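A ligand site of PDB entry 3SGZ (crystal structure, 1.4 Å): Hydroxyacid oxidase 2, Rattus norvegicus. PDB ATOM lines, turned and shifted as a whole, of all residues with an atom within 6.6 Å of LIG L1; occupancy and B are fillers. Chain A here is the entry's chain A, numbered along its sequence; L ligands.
OH of Tyr 129 sits at hydrogen-bond distance from N2 of LIG L1 (2.7 Å). The guanidinium group (NH2) of Arg 250 is in salt-bridge range of an oxygen (O2) of LIG L1 (2.8 Å). A ring nitrogen (NE2) of His 247 lies within hydrogen-bond range of an oxygen (O1) of LIG L1 (2.8 Å). An oxygen (O2) of LIG L1 lies within salt-bridge range of the guanidinium group of Arg 164 (2.9 Å). NE2 of His 247 lies close to N1 of LG2 L2 (3.5 Å). A nitrogen (N3) of LG2 L2 sits at hydrogen-bond distance from the backbone NH (N) of Ala 78 (3.0 Å). OE1 of Gln 127 is in hydrogen-bond range of N2 of LG2 L2, at 3.0 Å. OG of Ser 105 is in hydrogen-bond range of O2 of LG2 L2. An oxygen (O1) of LG2 L2 is in hydrogen-bond range of the side-chain hydroxyl (OG1) of Thr 155 (2.7 Å). The backbone carbonyl oxygen (O) of Pro 76 is in hydrogen-bond range of an oxygen (O3) of LG2 L2 (2.7 Å).
The guanidinium group of Arg 164 lies within hydrogen-bond range of the backbone carbonyl oxygen of Arg 250. The backbone carbonyl oxygen (O) of Phe 23 sits at hydrogen-bond distance from the guanidinium group (NH1) of Arg 250, 2.8 Å away. ND1 of His 247 lies close to OG1 of Thr 158. The guanidinium group (NH2) of Arg 164 sits close to the side-chain amide nitrogen (NE2) of Gln 251 (2.9 Å). The backbone NH (N) of Phe 79 is in hydrogen-bond range of the backbone carbonyl oxygen (O) of Tyr 107, 2.9 Å away. The backbone NH (N) of Tyr 107 sits at hydrogen-bond distance from the side-chain hydroxyl (OG) of Ser 105 (2.9 Å). The side-chain carboxylate (OD1) of Asp 167 sits close to the backbone NH (N) of Phe 23 (3.4 Å).
CE2 of Phe 23 touches O2 of LIG L1, 3.6 Å away. Phe 79 touches LIG L1. CG of Tyr 107 touches C6 of LIG L1 (3.5 Å). CD1 of Leu 161 touches C3 of LIG L1, at 3.8 Å. Leu 198 touches LIG L1. Phe 199 touches LIG L1 (CE1 to S2, 3.8 Å). Of the 18 residues printed, 10 come within 4 Å of LIG L1. The nearest printed residue that does not touch LIG L1 is Thr 158 (4.3 Å).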
ATOM      1  N   PHE A  23     -19.963 -19.953 -13.613  1.00  0.00           N
ATOM      2  CA  PHE A  23     -20.059 -18.531 -13.880  1.00  0.00           C
ATOM      3  C   PHE A  23     -20.117 -18.285 -15.398  1.00  0.00           C
ATOM      4  O   PHE A  23     -20.911 -17.441 -15.876  1.00  0.00           O
ATOM      5  CB  PHE A  23     -18.877 -17.787 -13.271  1.00  0.00           C
ATOM      6  CG  PHE A  23     -18.836 -16.344 -13.618  1.00  0.00           C
ATOM      7  CD1 PHE A  23     -17.837 -15.843 -14.445  1.00  0.00           C
ATOM      8  CD2 PHE A  23     -19.843 -15.494 -13.191  1.00  0.00           C
ATOM      9  CE1 PHE A  23     -17.829 -14.517 -14.851  1.00  0.00           C
ATOM     10  CE2 PHE A  23     -19.852 -14.154 -13.599  1.00  0.00           C
ATOM     11  CZ  PHE A  23     -18.859 -13.674 -14.423  1.00  0.00           C
ATOM     12  N   PRO A  76     -18.813  -7.918 -24.902  1.00  0.00           N
ATOM     13  CA  PRO A  76     -18.203  -7.655 -23.605  1.00  0.00           C
ATOM     14  C   PRO A  76     -18.462  -8.762 -22.620  1.00  0.00           C
ATOM     15  O   PRO A  76     -19.620  -9.125 -22.359  1.00  0.00           O
ATOM     16  CB  PRO A  76     -18.842  -6.313 -23.157  1.00  0.00           C
ATOM     17  CG  PRO A  76     -20.162  -6.293 -23.894  1.00  0.00           C
ATOM     18  CD  PRO A  76     -19.862  -6.943 -25.253  1.00  0.00           C
ATOM     19  N   ALA A  78     -17.009 -10.044 -18.715  1.00  0.00           N
ATOM     20  CA  ALA A  78     -16.151  -9.747 -17.558  1.00  0.00           C
ATOM     21  C   ALA A  78     -15.089 -10.779 -17.231  1.00  0.00           C
ATOM     22  O   ALA A  78     -15.211 -11.955 -17.568  1.00  0.00           O
ATOM     23  CB  ALA A  78     -17.035  -9.584 -16.345  1.00  0.00           C
ATOM     24  N   PHE A  79     -14.035 -10.289 -16.592  1.00  0.00           N
ATOM     25  CA  PHE A  79     -13.029 -11.164 -15.973  1.00  0.00           C
ATOM     26  C   PHE A  79     -12.369 -12.240 -16.799  1.00  0.00           C
ATOM     27  O   PHE A  79     -12.466 -13.429 -16.456  1.00  0.00           O
ATOM     28  CB  PHE A  79     -13.685 -11.855 -14.746  1.00  0.00           C
ATOM     29  CG  PHE A  79     -14.401 -10.915 -13.797  1.00  0.00           C
ATOM     30  CD1 PHE A  79     -15.709 -11.186 -13.386  1.00  0.00           C
ATOM     31  CD2 PHE A  79     -13.778  -9.797 -13.311  1.00  0.00           C
ATOM     32  CE1 PHE A  79     -16.370 -10.333 -12.489  1.00  0.00           C
ATOM     33  CE2 PHE A  79     -14.431  -8.926 -12.403  1.00  0.00           C
ATOM     34  CZ  PHE A  79     -15.712  -9.203 -12.010  1.00  0.00           C
ATOM     35  N   SER A 105     -15.061  -5.329 -21.595  1.00  0.00           N
ATOM     36  CA  SER A 105     -16.034  -5.212 -20.504  1.00  0.00           C
ATOM     37  C   SER A 105     -15.649  -4.162 -19.498  1.00  0.00           C
ATOM     38  O   SER A 105     -14.486  -3.837 -19.320  1.00  0.00           O
ATOM     39  CB  SER A 105     -16.158  -6.537 -19.762  1.00  0.00           C
ATOM     40  OG  SER A 105     -16.834  -6.422 -18.501  1.00  0.00           O
ATOM     41  N   TYR A 107     -15.775  -4.684 -16.499  1.00  0.00           N
ATOM     42  CA  TYR A 107     -15.179  -5.428 -15.392  1.00  0.00           C
ATOM     43  C   TYR A 107     -14.082  -6.339 -15.882  1.00  0.00           C
ATOM     44  O   TYR A 107     -14.093  -7.549 -15.649  1.00  0.00           O
ATOM     45  CB  TYR A 107     -16.230  -6.253 -14.687  1.00  0.00           C
ATOM     46  CG  TYR A 107     -17.169  -5.402 -13.890  1.00  0.00           C
ATOM     47  CD1 TYR A 107     -16.755  -4.846 -12.677  1.00  0.00           C
ATOM     48  CD2 TYR A 107     -18.462  -5.179 -14.323  1.00  0.00           C
ATOM     49  CE1 TYR A 107     -17.614  -4.079 -11.918  1.00  0.00           C
ATOM     50  CE2 TYR A 107     -19.343  -4.405 -13.567  1.00  0.00           C
ATOM     51  CZ  TYR A 107     -18.908  -3.865 -12.361  1.00  0.00           C
ATOM     52  OH  TYR A 107     -19.781  -3.146 -11.562  1.00  0.00           O
ATOM     53  N   GLN A 127     -17.365  -1.165 -23.086  1.00  0.00           N
ATOM     54  CA  GLN A 127     -18.679  -1.251 -22.468  1.00  0.00           C
ATOM     55  C   GLN A 127     -18.507  -0.748 -21.048  1.00  0.00           C
ATOM     56  O   GLN A 127     -17.759  -1.316 -20.268  1.00  0.00           O
ATOM     57  CB  GLN A 127     -19.154  -2.713 -22.482  1.00  0.00           C
ATOM     58  CG  GLN A 127     -20.563  -2.928 -21.884  1.00  0.00           C
ATOM     59  CD  GLN A 127     -20.521  -3.333 -20.416  1.00  0.00           C
ATOM     60  OE1 GLN A 127     -19.762  -4.233 -20.038  1.00  0.00           O
ATOM     61  NE2 GLN A 127     -21.328  -2.690 -19.570  1.00  0.00           N
ATOM     62  N   TYR A 129     -20.371   0.353 -17.418  1.00  0.00           N
ATOM     63  CA  TYR A 129     -21.527   0.431 -16.563  1.00  0.00           C
ATOM     64  C   TYR A 129     -21.353   1.775 -15.839  1.00  0.00           C
ATOM     65  O   TYR A 129     -20.330   2.012 -15.186  1.00  0.00           O
ATOM     66  CB  TYR A 129     -21.553  -0.715 -15.552  1.00  0.00           C
ATOM     67  CG  TYR A 129     -22.114  -1.985 -16.116  1.00  0.00           C
ATOM     68  CD1 TYR A 129     -21.331  -3.138 -16.201  1.00  0.00           C
ATOM     69  CD2 TYR A 129     -23.449  -2.060 -16.577  1.00  0.00           C
ATOM     70  CE1 TYR A 129     -21.839  -4.330 -16.719  1.00  0.00           C
ATOM     71  CE2 TYR A 129     -23.963  -3.243 -17.113  1.00  0.00           C
ATOM     72  CZ  TYR A 129     -23.149  -4.375 -17.174  1.00  0.00           C
ATOM     73  OH  TYR A 129     -23.610  -5.563 -17.702  1.00  0.00           O
ATOM     74  N   THR A 155     -24.789  -1.261 -21.790  1.00  0.00           N
ATOM     75  CA  THR A 155     -25.623  -2.476 -21.650  1.00  0.00           C
ATOM     76  C   THR A 155     -26.776  -2.068 -20.763  1.00  0.00           C
ATOM     77  O   THR A 155     -26.568  -1.556 -19.668  1.00  0.00           O
ATOM     78  CB  THR A 155     -24.797  -3.559 -21.019  1.00  0.00           C
ATOM     79  OG1 THR A 155     -23.780  -3.912 -21.952  1.00  0.00           O
ATOM     80  CG2 THR A 155     -25.675  -4.794 -20.733  1.00  0.00           C
ATOM     81  N   THR A 158     -29.138  -4.974 -17.430  1.00  0.00           N
ATOM     82  CA  THR A 158     -28.571  -5.375 -16.158  1.00  0.00           C
ATOM     83  C   THR A 158     -28.690  -4.315 -15.042  1.00  0.00           C
ATOM     84  O   THR A 158     -27.702  -3.922 -14.438  1.00  0.00           O
ATOM     85  CB  THR A 158     -27.088  -5.804 -16.390  1.00  0.00           C
ATOM     86  OG1 THR A 158     -27.069  -6.673 -17.532  1.00  0.00           O
ATOM     87  CG2 THR A 158     -26.503  -6.548 -15.171  1.00  0.00           C
ATOM     88  N   LEU A 161     -28.318  -7.780 -11.212  1.00  0.00           N
ATOM     89  CA  LEU A 161     -27.781  -9.001 -11.787  1.00  0.00           C
ATOM     90  C   LEU A 161     -28.844 -10.086 -11.824  1.00  0.00           C
ATOM     91  O   LEU A 161     -29.715 -10.163 -10.966  1.00  0.00           O
ATOM     92  CB  LEU A 161     -26.587  -9.534 -10.973  1.00  0.00           C
ATOM     93  CG  LEU A 161     -25.588 -10.346 -11.817  1.00  0.00           C
ATOM     94  CD1 LEU A 161     -24.691  -9.335 -12.565  1.00  0.00           C
ATOM     95  CD2 LEU A 161     -24.774 -11.282 -10.961  1.00  0.00           C
ATOM     96  N   ARG A 164     -28.693 -16.466 -10.977  1.00  0.00           N
ATOM     97  CA  ARG A 164     -28.048 -17.661 -11.532  1.00  0.00           C
ATOM     98  C   ARG A 164     -27.890 -18.632 -10.380  1.00  0.00           C
ATOM     99  O   ARG A 164     -27.014 -18.461  -9.510  1.00  0.00           O
ATOM    100  CB  ARG A 164     -26.721 -17.222 -12.142  1.00  0.00           C
ATOM    101  CG  ARG A 164     -26.985 -16.180 -13.220  1.00  0.00           C
ATOM    102  CD  ARG A 164     -25.818 -15.352 -13.493  1.00  0.00           C
ATOM    103  NE  ARG A 164     -26.138 -14.166 -14.276  1.00  0.00           N
ATOM    104  CZ  ARG A 164     -25.212 -13.323 -14.690  1.00  0.00           C
ATOM    105  NH1 ARG A 164     -23.922 -13.586 -14.378  1.00  0.00           N
ATOM    106  NH2 ARG A 164     -25.547 -12.216 -15.353  1.00  0.00           N
ATOM    107  N   ASP A 167     -24.355 -20.330  -9.465  1.00  0.00           N
ATOM    108  CA  ASP A 167     -23.461 -19.355  -8.845  1.00  0.00           C
ATOM    109  C   ASP A 167     -23.847 -19.120  -7.402  1.00  0.00           C
ATOM    110  O   ASP A 167     -22.981 -19.045  -6.535  1.00  0.00           O
ATOM    111  CB  ASP A 167     -23.531 -17.993  -9.507  1.00  0.00           C
ATOM    112  CG  ASP A 167     -22.849 -17.942 -10.833  1.00  0.00           C
ATOM    113  OD1 ASP A 167     -22.131 -18.893 -11.210  1.00  0.00           O
ATOM    114  OD2 ASP A 167     -23.032 -16.901 -11.522  1.00  0.00           O
ATOM    115  N   LEU A 198     -20.815  -7.712  -6.164  1.00  0.00           N
ATOM    116  CA  LEU A 198     -21.895  -6.709  -6.268  1.00  0.00           C
ATOM    117  C   LEU A 198     -21.576  -5.364  -6.928  1.00  0.00           C
ATOM    118  O   LEU A 198     -20.545  -4.690  -6.729  1.00  0.00           O
ATOM    119  CB  LEU A 198     -22.579  -6.510  -4.939  1.00  0.00           C
ATOM    120  N   PHE A 199     -22.608  -5.087  -7.710  1.00  0.00           N
ATOM    121  CA  PHE A 199     -23.004  -4.096  -8.709  1.00  0.00           C
ATOM    122  C   PHE A 199     -23.364  -2.556  -8.756  1.00  0.00           C
ATOM    123  O   PHE A 199     -22.443  -1.739  -8.824  1.00  0.00           O
ATOM    124  CB  PHE A 199     -24.067  -4.896  -9.390  1.00  0.00           C
ATOM    125  CG  PHE A 199     -24.086  -4.762 -10.832  1.00  0.00           C
ATOM    126  CD1 PHE A 199     -22.941  -4.926 -11.599  1.00  0.00           C
ATOM    127  CD2 PHE A 199     -25.286  -4.499 -11.447  1.00  0.00           C
ATOM    128  CE1 PHE A 199     -23.018  -4.824 -12.971  1.00  0.00           C
ATOM    129  CE2 PHE A 199     -25.372  -4.396 -12.789  1.00  0.00           C
ATOM    130  CZ  PHE A 199     -24.234  -4.564 -13.570  1.00  0.00           C
ATOM    131  N   HIS A 247     -28.501 -10.948 -23.201  1.00  0.00           N
ATOM    132  CA  HIS A 247     -27.404 -11.195 -22.247  1.00  0.00           C
ATOM    133  C   HIS A 247     -27.158 -12.694 -22.075  1.00  0.00           C
ATOM    134  O   HIS A 247     -26.805 -13.158 -20.992  1.00  0.00           O
ATOM    135  CB  HIS A 247     -27.733 -10.491 -20.907  1.00  0.00           C
ATOM    136  CG  HIS A 247     -26.531 -10.008 -20.122  1.00  0.00           C
ATOM    137  ND1 HIS A 247     -26.287  -8.663 -19.949  1.00  0.00           N
ATOM    138  CD2 HIS A 247     -25.567 -10.671 -19.418  1.00  0.00           C
ATOM    139  CE1 HIS A 247     -25.218  -8.516 -19.163  1.00  0.00           C
ATOM    140  NE2 HIS A 247     -24.771  -9.712 -18.838  1.00  0.00           N
ATOM    141  N   ARG A 250     -28.705 -14.830 -19.188  1.00  0.00           N
ATOM    142  CA  ARG A 250     -28.130 -14.689 -17.856  1.00  0.00           C
ATOM    143  C   ARG A 250     -28.863 -13.626 -16.997  1.00  0.00           C
ATOM    144  O   ARG A 250     -28.542 -13.486 -15.809  1.00  0.00           O
ATOM    145  CB  ARG A 250     -26.663 -14.226 -17.978  1.00  0.00           C
ATOM    146  CG  ARG A 250     -25.795 -15.225 -18.729  1.00  0.00           C
ATOM    147  CD  ARG A 250     -24.452 -14.617 -19.079  1.00  0.00           C
ATOM    148  NE  ARG A 250     -23.579 -14.257 -17.965  1.00  0.00           N
ATOM    149  CZ  ARG A 250     -22.767 -15.128 -17.363  1.00  0.00           C
ATOM    150  NH1 ARG A 250     -22.780 -16.397 -17.744  1.00  0.00           N
ATOM    151  NH2 ARG A 250     -21.837 -14.698 -16.508  1.00  0.00           N
ATOM    152  N   GLN A 251     -29.810 -12.904 -17.612  1.00  0.00           N
ATOM    153  CA  GLN A 251     -30.501 -11.818 -16.913  1.00  0.00           C
ATOM    154  C   GLN A 251     -31.976 -12.180 -16.740  1.00  0.00           C
ATOM    155  O   GLN A 251     -32.265 -13.099 -15.987  1.00  0.00           O
ATOM    156  CB  GLN A 251     -30.251 -10.531 -17.715  1.00  0.00           C
ATOM    157  CG  GLN A 251     -28.795 -10.020 -17.514  1.00  0.00           C
ATOM    158  CD  GLN A 251     -28.608  -9.610 -16.084  1.00  0.00           C
ATOM    159  OE1 GLN A 251     -29.347  -8.709 -15.564  1.00  0.00           O
ATOM    160  NE2 GLN A 251     -27.686 -10.234 -15.402  1.00  0.00           N
HETATM  161  C1  LIG L   1     -19.750  -7.299 -10.477  1.00  0.00           C
HETATM  162  N1  LIG L   1     -22.776  -8.808 -16.788  1.00  0.00           N
HETATM  163  O1  LIG L   1     -23.268 -11.460 -17.241  1.00  0.00           O
HETATM  164  S1  LIG L   1     -20.714 -10.389 -13.733  1.00  0.00           S
HETATM  165  C2  LIG L   1     -20.833  -8.167 -10.275  1.00  0.00           C
HETATM  166  N2  LIG L   1     -22.467  -7.569 -16.290  1.00  0.00           N
HETATM  167  O2  LIG L   1     -21.871 -12.071 -15.687  1.00  0.00           O
HETATM  168  S2  LIG L   1     -21.490  -7.656 -14.927  1.00  0.00           S
HETATM  169  C3  LIG L   1     -21.138  -9.128 -11.271  1.00  0.00           C
HETATM  170  C4  LIG L   1     -20.365  -9.194 -12.454  1.00  0.00           C
HETATM  171  C5  LIG L   1     -19.284  -8.317 -12.624  1.00  0.00           C
HETATM  172  C6  LIG L   1     -18.967  -7.365 -11.631  1.00  0.00           C
HETATM  173  C7  LIG L   1     -21.300  -9.337 -15.116  1.00  0.00           C
HETATM  174  C8  LIG L   1     -22.132  -9.838 -16.016  1.00  0.00           C
HETATM  175  C9  LIG L   1     -22.445 -11.214 -16.338  1.00  0.00           C
HETATM  176  C10 LIG L   1     -19.321  -6.116  -9.328  1.00  0.00           C
HETATM  177  N1  LG2 L   2     -22.362  -8.439 -20.978  1.00  0.00           N
HETATM  178  C1  LG2 L   2     -22.059  -7.119 -20.788  1.00  0.00           C
HETATM  179  O1  LG2 L   2     -22.618  -6.255 -21.409  1.00  0.00           O
HETATM  180  N2  LG2 L   2     -21.034  -6.891 -19.835  1.00  0.00           N
HETATM  181  C2  LG2 L   2     -20.333  -7.839 -19.112  1.00  0.00           C
HETATM  182  O2  LG2 L   2     -19.460  -7.438 -18.340  1.00  0.00           O
HETATM  183  C3  LG2 L   2     -20.728  -9.155 -19.402  1.00  0.00           C
HETATM  184  N3  LG2 L   2     -20.005 -10.138 -18.727  1.00  0.00           N
HETATM  185  C4  LG2 L   2     -20.278 -11.463 -19.076  1.00  0.00           C
HETATM  186  C5  LG2 L   2     -19.510 -12.456 -18.467  1.00  0.00           C
HETATM  187  C6  LG2 L   2     -19.673 -13.781 -18.870  1.00  0.00           C
HETATM  188  C7  LG2 L   2     -18.787 -14.838 -18.224  1.00  0.00           C
HETATM  189  C8  LG2 L   2     -20.625 -14.114 -19.859  1.00  0.00           C
HETATM  190  C9  LG2 L   2     -20.794 -15.521 -20.351  1.00  0.00           C
HETATM  191  C10 LG2 L   2     -21.432 -13.145 -20.449  1.00  0.00           C
HETATM  192  C11 LG2 L   2     -21.277 -11.796 -20.067  1.00  0.00           C
HETATM  193  N4  LG2 L   2     -22.026 -10.753 -20.679  1.00  0.00           N
HETATM  194  C12 LG2 L   2     -21.733  -9.451 -20.361  1.00  0.00           C
HETATM  195  C13 LG2 L   2     -23.016 -11.001 -21.677  1.00  0.00           C
HETATM  196  C14 LG2 L   2     -22.331 -11.223 -23.094  1.00  0.00           C
HETATM  197  O3  LG2 L   2     -21.916  -9.933 -23.601  1.00  0.00           O
HETATM  198  C15 LG2 L   2     -23.217 -11.830 -24.150  1.00  0.00           C
HETATM  199  O4  LG2 L   2     -24.434 -10.954 -24.240  1.00  0.00           O
HETATM  200  C16 LG2 L   2     -23.736 -13.151 -23.848  1.00  0.00           C
HETATM  201  O5  LG2 L   2     -22.697 -14.043 -23.347  1.00  0.00           O
HETATM  202  C17 LG2 L   2     -24.502 -13.836 -25.004  1.00  0.00           C
HETATM  203  O6  LG2 L   2     -23.567 -14.291 -26.074  1.00  0.00           O
HETATM  204  P1  LG2 L   2     -23.121 -15.839 -26.141  1.00  0.00           P
HETATM  205  O7  LG2 L   2     -24.349 -16.670 -26.387  1.00  0.00           O
HETATM  206  O8  LG2 L   2     -22.453 -16.235 -24.849  1.00  0.00           O
HETATM  207  O9  LG2 L   2     -22.221 -15.828 -27.308  1.00  0.00           O
